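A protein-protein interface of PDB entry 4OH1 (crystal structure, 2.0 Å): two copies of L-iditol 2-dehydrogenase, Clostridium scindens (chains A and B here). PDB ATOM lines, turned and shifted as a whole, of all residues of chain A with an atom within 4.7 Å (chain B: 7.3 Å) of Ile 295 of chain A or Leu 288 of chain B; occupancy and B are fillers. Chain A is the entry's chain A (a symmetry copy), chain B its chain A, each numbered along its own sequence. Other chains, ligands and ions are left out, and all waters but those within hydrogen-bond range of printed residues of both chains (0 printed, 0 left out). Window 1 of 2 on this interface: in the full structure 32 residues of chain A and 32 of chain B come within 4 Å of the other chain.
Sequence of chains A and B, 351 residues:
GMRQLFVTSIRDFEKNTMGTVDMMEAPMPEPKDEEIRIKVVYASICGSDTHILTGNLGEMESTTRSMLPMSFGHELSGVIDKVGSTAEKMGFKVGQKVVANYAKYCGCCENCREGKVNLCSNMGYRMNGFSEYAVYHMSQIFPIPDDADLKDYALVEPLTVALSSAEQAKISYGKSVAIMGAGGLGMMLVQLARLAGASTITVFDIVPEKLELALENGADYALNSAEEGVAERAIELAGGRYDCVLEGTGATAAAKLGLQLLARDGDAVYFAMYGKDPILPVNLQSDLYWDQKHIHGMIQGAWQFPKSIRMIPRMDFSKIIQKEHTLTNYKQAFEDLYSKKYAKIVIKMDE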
ATOM      1  N   LEU A 259     -32.716 -14.805  24.454  1.00  0.00           N
ATOM      2  CA  LEU A 259     -32.024 -13.518  24.319  1.00  0.00           C
ATOM      3  C   LEU A 259     -33.000 -12.367  24.542  1.00  0.00           C
ATOM      4  O   LEU A 259     -32.682 -11.350  25.185  1.00  0.00           O
ATOM      5  CB  LEU A 259     -31.364 -13.414  22.945  1.00  0.00           C
ATOM      6  CG  LEU A 259     -30.471 -12.217  22.662  1.00  0.00           C
ATOM      7  CD1 LEU A 259     -29.285 -12.167  23.584  1.00  0.00           C
ATOM      8  CD2 LEU A 259     -29.995 -12.308  21.192  1.00  0.00           C
ATOM      9  N   ALA A 268     -26.714 -14.681  29.569  1.00  0.00           N
ATOM     10  CA  ALA A 268     -27.350 -15.852  28.896  1.00  0.00           C
ATOM     11  C   ALA A 268     -26.305 -16.921  28.575  1.00  0.00           C
ATOM     12  O   ALA A 268     -25.262 -16.608  27.963  1.00  0.00           O
ATOM     13  CB  ALA A 268     -28.016 -15.425  27.624  1.00  0.00           C
ATOM     14  N   TYR A 270     -25.731 -20.655  26.718  1.00  0.00           N
ATOM     15  CA  TYR A 270     -26.149 -21.603  25.707  1.00  0.00           C
ATOM     16  C   TYR A 270     -25.279 -22.819  25.847  1.00  0.00           C
ATOM     17  O   TYR A 270     -24.147 -22.838  25.419  1.00  0.00           O
ATOM     18  CB  TYR A 270     -26.039 -20.951  24.315  1.00  0.00           C
ATOM     19  CG  TYR A 270     -27.006 -19.809  24.163  1.00  0.00           C
ATOM     20  CD1 TYR A 270     -28.316 -20.011  23.759  1.00  0.00           C
ATOM     21  CD2 TYR A 270     -26.629 -18.517  24.477  1.00  0.00           C
ATOM     22  CE1 TYR A 270     -29.231 -18.932  23.637  1.00  0.00           C
ATOM     23  CE2 TYR A 270     -27.520 -17.455  24.376  1.00  0.00           C
ATOM     24  CZ  TYR A 270     -28.811 -17.664  23.935  1.00  0.00           C
ATOM     25  OH  TYR A 270     -29.665 -16.596  23.893  1.00  0.00           O
ATOM     26  N   VAL A 282     -27.664 -11.773  16.578  1.00  0.00           N
ATOM     27  CA  VAL A 282     -27.524 -10.868  17.678  1.00  0.00           C
ATOM     28  C   VAL A 282     -27.557  -9.515  17.086  1.00  0.00           C
ATOM     29  O   VAL A 282     -26.884  -9.255  16.099  1.00  0.00           O
ATOM     30  CB  VAL A 282     -26.240 -11.092  18.451  1.00  0.00           C
ATOM     31  CG1 VAL A 282     -26.087 -10.032  19.501  1.00  0.00           C
ATOM     32  CG2 VAL A 282     -26.304 -12.436  19.135  1.00  0.00           C
ATOM     33  N   LEU A 288     -26.492  -5.517  22.421  1.00  0.00           N
ATOM     34  CA  LEU A 288     -25.176  -5.342  22.959  1.00  0.00           C
ATOM     35  C   LEU A 288     -24.898  -3.897  23.318  1.00  0.00           C
ATOM     36  O   LEU A 288     -24.689  -3.606  24.468  1.00  0.00           O
ATOM     37  CB  LEU A 288     -24.093  -5.876  21.986  1.00  0.00           C
ATOM     38  CG  LEU A 288     -24.195  -7.376  21.687  1.00  0.00           C
ATOM     39  CD1 LEU A 288     -22.917  -7.927  21.030  1.00  0.00           C
ATOM     40  CD2 LEU A 288     -24.557  -8.192  22.906  1.00  0.00           C
ATOM     41  N   LYS A 293     -25.832  -6.820  27.032  1.00  0.00           N
ATOM     42  CA  LYS A 293     -26.042  -8.228  27.304  1.00  0.00           C
ATOM     43  C   LYS A 293     -24.722  -9.020  27.263  1.00  0.00           C
ATOM     44  O   LYS A 293     -23.730  -8.571  26.722  1.00  0.00           O
ATOM     45  CB  LYS A 293     -27.093  -8.823  26.384  1.00  0.00           C
ATOM     46  CG  LYS A 293     -28.499  -8.280  26.606  1.00  0.00           C
ATOM     47  CD  LYS A 293     -29.411  -8.688  25.465  1.00  0.00           C
ATOM     48  CE  LYS A 293     -30.844  -8.217  25.735  1.00  0.00           C
ATOM     49  NZ  LYS A 293     -31.733  -8.795  24.714  1.00  0.00           N
ATOM     50  N   HIS A 294     -24.695 -10.136  27.983  1.00  0.00           N
ATOM     51  CA  HIS A 294     -23.536 -11.019  27.997  1.00  0.00           C
ATOM     52  C   HIS A 294     -24.056 -12.367  27.539  1.00  0.00           C
ATOM     53  O   HIS A 294     -25.004 -12.909  28.143  1.00  0.00           O
ATOM     54  CB  HIS A 294     -22.882 -11.122  29.376  1.00  0.00           C
ATOM     55  CG  HIS A 294     -22.699  -9.810  30.052  1.00  0.00           C
ATOM     56  ND1 HIS A 294     -21.635  -8.993  29.801  1.00  0.00           N
ATOM     57  CD2 HIS A 294     -23.464  -9.159  30.955  1.00  0.00           C
ATOM     58  CE1 HIS A 294     -21.762  -7.875  30.497  1.00  0.00           C
ATOM     59  NE2 HIS A 294     -22.866  -7.951  31.196  1.00  0.00           N
ATOM     60  N   ILE A 295     -23.445 -12.870  26.457  1.00  0.00           N
ATOM     61  CA  ILE A 295     -23.828 -14.150  25.846  1.00  0.00           C
ATOM     62  C   ILE A 295     -22.658 -15.126  25.957  1.00  0.00           C
ATOM     63  O   ILE A 295     -21.544 -14.841  25.478  1.00  0.00           O
ATOM     64  CB  ILE A 295     -24.153 -13.882  24.373  1.00  0.00           C
ATOM     65  CG1 ILE A 295     -25.406 -12.995  24.320  1.00  0.00           C
ATOM     66  CG2 ILE A 295     -24.372 -15.181  23.620  1.00  0.00           C
ATOM     67  CD1 ILE A 295     -25.660 -12.428  22.987  1.00  0.00           C
ATOM     68  N   HIS A 296     -22.914 -16.258  26.568  1.00  0.00           N
ATOM     69  CA  HIS A 296     -21.869 -17.220  26.851  1.00  0.00           C
ATOM     70  C   HIS A 296     -22.201 -18.580  26.312  1.00  0.00           C
ATOM     71  O   HIS A 296     -23.376 -19.020  26.315  1.00  0.00           O
ATOM     72  CB  HIS A 296     -21.723 -17.464  28.356  1.00  0.00           C
ATOM     73  CG  HIS A 296     -21.662 -16.230  29.175  1.00  0.00           C
ATOM     74  ND1 HIS A 296     -20.510 -15.496  29.323  1.00  0.00           N
ATOM     75  CD2 HIS A 296     -22.601 -15.607  29.930  1.00  0.00           C
ATOM     76  CE1 HIS A 296     -20.743 -14.464  30.116  1.00  0.00           C
ATOM     77  NE2 HIS A 296     -22.006 -14.502  30.484  1.00  0.00           N
ATOM     78  N   GLY A 297     -21.146 -19.278  25.930  1.00  0.00           N
ATOM     79  CA  GLY A 297     -21.207 -20.716  25.764  1.00  0.00           C
ATOM     80  C   GLY A 297     -20.726 -21.481  27.002  1.00  0.00           C
ATOM     81  O   GLY A 297     -20.304 -20.899  28.012  1.00  0.00           O
ATOM     82  N   MET A 298     -20.773 -22.806  26.902  1.00  0.00           N
ATOM     83  CA  MET A 298     -20.422 -23.717  28.000  1.00  0.00           C
ATOM     84  C   MET A 298     -20.035 -25.102  27.402  1.00  0.00           C
ATOM     85  O   MET A 298     -20.896 -25.807  26.837  1.00  0.00           O
ATOM     86  CB  MET A 298     -21.625 -23.845  28.953  1.00  0.00           C
ATOM     87  CG  MET A 298     -21.267 -23.892  30.462  1.00  0.00           C
ATOM     88  SD  MET A 298     -20.181 -25.446  30.814  1.00  0.00           S
ATOM     89  CE  MET A 298     -21.652 -26.774  30.649  1.00  0.00           C
ATOM     90  N   LEU B 259     -15.381 -11.908  15.924  1.00  0.00           N
ATOM     91  CA  LEU B 259     -15.855 -13.165  16.514  1.00  0.00           C
ATOM     92  C   LEU B 259     -15.014 -14.334  16.011  1.00  0.00           C
ATOM     93  O   LEU B 259     -14.660 -15.261  16.762  1.00  0.00           O
ATOM     94  CB  LEU B 259     -17.332 -13.379  16.188  1.00  0.00           C
ATOM     95  CG  LEU B 259     -18.051 -14.552  16.835  1.00  0.00           C
ATOM     96  CD1 LEU B 259     -18.072 -14.446  18.334  1.00  0.00           C
ATOM     97  CD2 LEU B 259     -19.498 -14.591  16.286  1.00  0.00           C
ATOM     98  N   GLY B 266     -12.612 -17.047  25.007  1.00  0.00           N
ATOM     99  CA  GLY B 266     -12.236 -15.648  24.891  1.00  0.00           C
ATOM    100  C   GLY B 266     -13.390 -14.676  25.132  1.00  0.00           C
ATOM    101  O   GLY B 266     -14.550 -15.089  25.177  1.00  0.00           O
ATOM    102  N   ALA B 268     -15.143 -11.196  23.775  1.00  0.00           N
ATOM    103  CA  ALA B 268     -15.329 -10.135  22.741  1.00  0.00           C
ATOM    104  C   ALA B 268     -16.285  -9.054  23.245  1.00  0.00           C
ATOM    105  O   ALA B 268     -17.398  -9.376  23.712  1.00  0.00           O
ATOM    106  CB  ALA B 268     -15.882 -10.725  21.480  1.00  0.00           C
ATOM    107  N   VAL B 282     -24.523 -15.488  15.305  1.00  0.00           N
ATOM    108  CA  VAL B 282     -23.708 -16.264  16.189  1.00  0.00           C
ATOM    109  C   VAL B 282     -24.080 -17.672  15.939  1.00  0.00           C
ATOM    110  O   VAL B 282     -25.257 -17.999  15.880  1.00  0.00           O
ATOM    111  CB  VAL B 282     -23.919 -15.897  17.644  1.00  0.00           C
ATOM    112  CG1 VAL B 282     -23.144 -16.833  18.522  1.00  0.00           C
ATOM    113  CG2 VAL B 282     -23.414 -14.493  17.877  1.00  0.00           C
ATOM    114  N   ASN B 283     -23.073 -18.522  15.755  1.00  0.00           N
ATOM    115  CA  ASN B 283     -23.337 -19.928  15.598  1.00  0.00           C
ATOM    116  C   ASN B 283     -23.322 -20.596  16.956  1.00  0.00           C
ATOM    117  O   ASN B 283     -22.288 -20.691  17.600  1.00  0.00           O
ATOM    118  CB  ASN B 283     -22.333 -20.559  14.653  1.00  0.00           C
ATOM    119  CG  ASN B 283     -22.675 -21.967  14.318  1.00  0.00           C
ATOM    120  OD1 ASN B 283     -22.806 -22.828  15.191  1.00  0.00           O
ATOM    121  ND2 ASN B 283     -22.822 -22.240  13.030  1.00  0.00           N
ATOM    122  N   LEU B 284     -24.485 -21.071  17.380  1.00  0.00           N
ATOM    123  CA  LEU B 284     -24.671 -21.657  18.699  1.00  0.00           C
ATOM    124  C   LEU B 284     -23.788 -22.858  18.921  1.00  0.00           C
ATOM    125  O   LEU B 284     -23.270 -23.076  20.019  1.00  0.00           O
ATOM    126  CB  LEU B 284     -26.142 -22.044  18.875  1.00  0.00           C
ATOM    127  CG  LEU B 284     -27.039 -20.792  18.913  1.00  0.00           C
ATOM    128  CD1 LEU B 284     -28.433 -21.174  18.693  1.00  0.00           C
ATOM    129  CD2 LEU B 284     -26.903 -20.049  20.241  1.00  0.00           C
ATOM    130  N   GLN B 285     -23.642 -23.648  17.874  1.00  0.00           N
ATOM    131  CA  GLN B 285     -22.858 -24.881  17.930  1.00  0.00           C
ATOM    132  C   GLN B 285     -21.389 -24.570  17.955  1.00  0.00           C
ATOM    133  O   GLN B 285     -20.683 -25.076  18.778  1.00  0.00           O
ATOM    134  CB  GLN B 285     -23.150 -25.800  16.730  1.00  0.00           C
ATOM    135  CG  GLN B 285     -22.364 -27.119  16.744  1.00  0.00           C
ATOM    136  CD  GLN B 285     -22.932 -28.135  17.762  1.00  0.00           C
ATOM    137  OE1 GLN B 285     -24.001 -27.927  18.357  1.00  0.00           O
ATOM    138  NE2 GLN B 285     -22.205 -29.236  17.969  1.00  0.00           N
ATOM    139  N   SER B 286     -20.899 -23.762  17.035  1.00  0.00           N
ATOM    140  CA  SER B 286     -19.449 -23.633  16.961  1.00  0.00           C
ATOM    141  C   SER B 286     -18.880 -22.485  17.817  1.00  0.00           C
ATOM    142  O   SER B 286     -17.899 -22.678  18.530  1.00  0.00           O
ATOM    143  CB  SER B 286     -19.022 -23.516  15.511  1.00  0.00           C
ATOM    144  OG  SER B 286     -19.545 -22.330  15.011  1.00  0.00           O
ATOM    145  N   ASP B 287     -19.498 -21.311  17.769  1.00  0.00           N
ATOM    146  CA  ASP B 287     -19.055 -20.214  18.616  1.00  0.00           C
ATOM    147  C   ASP B 287     -19.258 -20.450  20.119  1.00  0.00           C
ATOM    148  O   ASP B 287     -18.366 -20.198  20.905  1.00  0.00           O
ATOM    149  CB  ASP B 287     -19.739 -18.922  18.205  1.00  0.00           C
ATOM    150  CG  ASP B 287     -19.395 -18.502  16.790  1.00  0.00           C
ATOM    151  OD1 ASP B 287     -18.197 -18.479  16.463  1.00  0.00           O
ATOM    152  OD2 ASP B 287     -20.329 -18.186  16.043  1.00  0.00           O
ATOM    153  N   LEU B 288     -20.389 -21.033  20.484  1.00  0.00           N
ATOM    154  CA  LEU B 288     -20.784 -21.084  21.860  1.00  0.00           C
ATOM    155  C   LEU B 288     -20.606 -22.468  22.449  1.00  0.00           C
ATOM    156  O   LEU B 288     -19.826 -22.627  23.354  1.00  0.00           O
ATOM    157  CB  LEU B 288     -22.246 -20.601  22.046  1.00  0.00           C
ATOM    158  CG  LEU B 288     -22.490 -19.147  21.625  1.00  0.00           C
ATOM    159  CD1 LEU B 288     -23.829 -18.604  22.157  1.00  0.00           C
ATOM    160  CD2 LEU B 288     -21.355 -18.227  22.013  1.00  0.00           C
ATOM    161  N   TYR B 289     -21.347 -23.454  21.976  1.00  0.00           N
ATOM    162  CA  TYR B 289     -21.205 -24.773  22.537  1.00  0.00           C
ATOM    163  C   TYR B 289     -19.741 -25.286  22.428  1.00  0.00           C
ATOM    164  O   TYR B 289     -19.155 -25.575  23.455  1.00  0.00           O
ATOM    165  CB  TYR B 289     -22.199 -25.740  21.924  1.00  0.00           C
ATOM    166  CG  TYR B 289     -21.919 -27.147  22.340  1.00  0.00           C
ATOM    167  CD1 TYR B 289     -22.239 -27.594  23.619  1.00  0.00           C
ATOM    168  CD2 TYR B 289     -21.273 -28.015  21.476  1.00  0.00           C
ATOM    169  CE1 TYR B 289     -21.968 -28.851  23.988  1.00  0.00           C
ATOM    170  CE2 TYR B 289     -20.991 -29.284  21.838  1.00  0.00           C
ATOM    171  CZ  TYR B 289     -21.331 -29.699  23.087  1.00  0.00           C
ATOM    172  OH  TYR B 289     -21.030 -30.985  23.414  1.00  0.00           O
ATOM    173  N   TRP B 290     -19.138 -25.344  21.240  1.00  0.00           N
ATOM    174  CA  TRP B 290     -17.794 -25.945  21.130  1.00  0.00           C
ATOM    175  C   TRP B 290     -16.747 -24.988  21.641  1.00  0.00           C
ATOM    176  O   TRP B 290     -15.909 -25.397  22.412  1.00  0.00           O
ATOM    177  CB  TRP B 290     -17.414 -26.534  19.731  1.00  0.00           C
ATOM    178  CG  TRP B 290     -16.058 -27.266  19.813  1.00  0.00           C
ATOM    179  CD1 TRP B 290     -14.867 -26.808  19.371  1.00  0.00           C
ATOM    180  CD2 TRP B 290     -15.781 -28.515  20.471  1.00  0.00           C
ATOM    181  NE1 TRP B 290     -13.871 -27.685  19.680  1.00  0.00           N
ATOM    182  CE2 TRP B 290     -14.408 -28.750  20.349  1.00  0.00           C
ATOM    183  CE3 TRP B 290     -16.570 -29.467  21.123  1.00  0.00           C
ATOM    184  CZ2 TRP B 290     -13.800 -29.874  20.872  1.00  0.00           C
ATOM    185  CZ3 TRP B 290     -15.967 -30.585  21.628  1.00  0.00           C
ATOM    186  CH2 TRP B 290     -14.601 -30.779  21.505  1.00  0.00           C
ATOM    187  N   ASP B 291     -16.817 -23.711  21.275  1.00  0.00           N
ATOM    188  CA  ASP B 291     -15.762 -22.756  21.624  1.00  0.00           C
ATOM    189  C   ASP B 291     -15.898 -21.960  22.947  1.00  0.00           C
ATOM    190  O   ASP B 291     -14.952 -21.303  23.389  1.00  0.00           O
ATOM    191  CB  ASP B 291     -15.492 -21.819  20.424  1.00  0.00           C
ATOM    192  CG  ASP B 291     -14.649 -22.503  19.348  1.00  0.00           C
ATOM    193  OD1 ASP B 291     -14.188 -23.655  19.570  1.00  0.00           O
ATOM    194  OD2 ASP B 291     -14.452 -21.876  18.305  1.00  0.00           O
ATOM    195  N   GLN B 292     -17.054 -22.031  23.590  1.00  0.00           N
ATOM    196  CA  GLN B 292     -17.217 -21.404  24.843  1.00  0.00           C
ATOM    197  C   GLN B 292     -16.850 -19.891  24.768  1.00  0.00           C
ATOM    198  O   GLN B 292     -16.190 -19.349  25.636  1.00  0.00           O
ATOM    199  CB  GLN B 292     -16.382 -22.167  25.902  1.00  0.00           C
ATOM    200  CG  GLN B 292     -16.871 -21.834  27.321  1.00  0.00           C
ATOM    201  CD  GLN B 292     -16.313 -22.710  28.419  1.00  0.00           C
ATOM    202  OE1 GLN B 292     -16.848 -23.785  28.716  1.00  0.00           O
ATOM    203  NE2 GLN B 292     -15.230 -22.240  29.048  1.00  0.00           N
ATOM    204  N   LYS B 293     -17.276 -19.224  23.713  1.00  0.00           N
ATOM    205  CA  LYS B 293     -17.003 -17.808  23.571  1.00  0.00           C
ATOM    206  C   LYS B 293     -17.900 -16.959  24.491  1.00  0.00           C
ATOM    207  O   LYS B 293     -18.919 -17.412  24.976  1.00  0.00           O
ATOM    208  CB  LYS B 293     -17.093 -17.365  22.121  1.00  0.00           C
ATOM    209  CG  LYS B 293     -16.014 -17.953  21.220  1.00  0.00           C
ATOM    210  CD  LYS B 293     -16.353 -17.712  19.762  1.00  0.00           C
ATOM    211  CE  LYS B 293     -15.223 -18.224  18.862  1.00  0.00           C
ATOM    212  NZ  LYS B 293     -15.492 -17.800  17.478  1.00  0.00           N
ATOM    213  N   HIS B 294     -17.412 -15.774  24.841  1.00  0.00           N
ATOM    214  CA  HIS B 294     -18.170 -14.837  25.660  1.00  0.00           C
ATOM    215  C   HIS B 294     -18.269 -13.572  24.832  1.00  0.00           C
ATOM    216  O   HIS B 294     -17.234 -13.019  24.410  1.00  0.00           O
ATOM    217  CB  HIS B 294     -17.510 -14.558  27.012  1.00  0.00           C
ATOM    218  CG  HIS B 294     -17.032 -15.782  27.709  1.00  0.00           C
ATOM    219  ND1 HIS B 294     -17.851 -16.566  28.469  1.00  0.00           N
ATOM    220  CD2 HIS B 294     -15.818 -16.372  27.740  1.00  0.00           C
ATOM    221  CE1 HIS B 294     -17.173 -17.610  28.917  1.00  0.00           C
ATOM    222  NE2 HIS B 294     -15.942 -17.517  28.480  1.00  0.00           N
ATOM    223  N   ILE B 295     -19.520 -13.155  24.586  1.00  0.00           N
ATOM    224  CA  ILE B 295     -19.820 -11.966  23.776  1.00  0.00           C
ATOM    225  C   ILE B 295     -20.514 -10.927  24.654  1.00  0.00           C
ATOM    226  O   ILE B 295     -21.569 -11.204  25.256  1.00  0.00           O
ATOM    227  CB  ILE B 295     -20.751 -12.402  22.640  1.00  0.00           C
ATOM    228  CG1 ILE B 295     -19.965 -13.352  21.724  1.00  0.00           C
ATOM    229  CG2 ILE B 295     -21.266 -11.202  21.868  1.00  0.00           C
ATOM    230  CD1 ILE B 295     -20.816 -14.067  20.761  1.00  0.00           C
ATOM    231  N   HIS B 296     -19.935  -9.751  24.715  1.00  0.00           N
ATOM    232  CA  HIS B 296     -20.416  -8.714  25.603  1.00  0.00           C
ATOM    233  C   HIS B 296     -20.697  -7.436  24.870  1.00  0.00           C
ATOM    234  O   HIS B 296     -19.982  -7.058  23.910  1.00  0.00           O
ATOM    235  CB  HIS B 296     -19.348  -8.307  26.622  1.00  0.00           C
ATOM    236  CG  HIS B 296     -18.686  -9.445  27.305  1.00  0.00           C
ATOM    237  ND1 HIS B 296     -19.253 -10.100  28.370  1.00  0.00           N
ATOM    238  CD2 HIS B 296     -17.479 -10.032  27.105  1.00  0.00           C
ATOM    239  CE1 HIS B 296     -18.438 -11.054  28.787  1.00  0.00           C
ATOM    240  NE2 HIS B 296     -17.364 -11.042  28.027  1.00  0.00           N
ATOM    241  N   GLY B 297     -21.689  -6.730  25.383  1.00  0.00           N
ATOM    242  CA  GLY B 297     -21.852  -5.322  25.082  1.00  0.00           C
ATOM    243  C   GLY B 297     -21.227  -4.409  26.142  1.00  0.00           C
ATOM    244  O   GLY B 297     -20.675  -4.860  27.156  1.00  0.00           O
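ND1 of His 296 of chain A lies within hydrogen-bond range of ND1 of His 294 of chain B. The backbone carbonyl oxygen (O) of Lys 293 of chain A is in hydrogen-bond range of the backbone NH (N) of Gly 297 of chain B (3.1 Å). O of Lys 293 of chain B lies within hydrogen-bond range of N of Gly 297 of chain A. The backbone carbonyl oxygen (O) of Ile 295 of chain A is in hydrogen-bond range of the backbone NH (N) of Ile 295 of chain B (2.8 Å). A ring nitrogen (ND1) of His 294 of chain A sits at hydrogen-bond distance from a ring nitrogen (ND1) of His 296 of chain B, at 3.0 Å.
O of Gln 292 of chain B is in hydrogen-bond range of NE2 of His 294 of chain B (3.4 Å). NZ of Lys 293 of chain B is in salt-bridge range of OD1 of Asp 287 of chain B (3.0 Å). N of Tyr 270 of chain A sits at hydrogen-bond distance from O of His 296 of chain A, at 2.9 Å. O of Leu 284 of chain B lies within hydrogen-bond range of N of Tyr 289 of chain B (2.8 Å). The backbone carbonyl oxygen (O) of Gly 266 of chain B lies within hydrogen-bond range of the backbone NH (N) of His 294 of chain B (3.0 Å). O of Leu 259 of chain B lies within hydrogen-bond range of NZ of Lys 293 of chain B (2.8 Å).
CG2 of Val 282 of chain B touches CG2 of Val 282 of chain A, at 3.8 Å. Leu 288 of chain A touches Ile 295 of chain B (CD1 to CG2, 3.8 Å). Gly 297 of chain B touches Leu 288 of chain A (CA to O, 3.4 Å). Ile 295 of chain B touches His 294 of chain A (O to CA, 3.4 Å). O of Ile 295 of chain A touches CA of His 294 of chain B (3.4 Å). His 296 of chain A touches Lys 293 of chain B. O of Leu 288 of chain B touches CA of Gly 297 of chain A (3.4 Å). O of Gly 297 of chain A touches CG of Gln 292 of chain B (3.6 Å). O of Tyr 289 of chain B touches O of Met 298 of chain A, at 3.8 Å. Gln 292 of chain B touches Met 298 of chain A (OE1 to CA, 3.6 Å).
Ile 295 of chain A touches just these residues of chain B: Leu 288, Lys 293, His 294 and Ile 295. Of chain A, only Tyr 270 (3.6 Å), Ile 295 (3.8 Å), Gly 297 (3.4 Å) and Met 298 (3.7 Å) come within 4 Å of Leu 288 of chain B. Printed residues of chain A within 4 Å of Gln 292 of chain B: Gly 297 (3.6 Å) and Met 298 (3.6 Å). Of the printed residues of chain B, Val 282 of chain A touches Val 282 (3.8 Å). Printed residues of chain B within 4 Å of Gly 297 of chain A: Leu 288 (3.4 Å), Gln 292 (3.6 Å) and Lys 293 (3.1 Å). The nearest residue of chain B that does not touch Ile 295 of chain A is His 296 of chain B (5.0 Å).
Printed residues of chain A that touch a printed residue of chain B: Tyr 270, Val 282, Leu 288, Lys 293, His 294, Ile 295, His 296, Gly 297 and Met 298. Hydrophobic or aromatic side chains of chain B within 4 Å of the printed part of chain A: Val 282, Leu 284, Leu 288, Tyr 289, His 294, Ile 295 and His 296. Among the printed residues, 22 pairs touch across the chains.
Val 282 of chain A touches its own counterpart, Val 282 of chain B. Leu 288 of chain A touches Gly 297 of chain B, and with the chains exchanged Gly 297 of chain A touches Leu 288 of chain B. Lys 293 of chain A touches Ile 295 of chain B, and with the chains exchanged Ile 295 of chain A touches Lys 293 of chain B. Lys 293 of chain A touches His 296 of chain B, and with the chains exchanged His 296 of chain A touches Lys 293 of chain B. 9 positions are printed for both chains.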
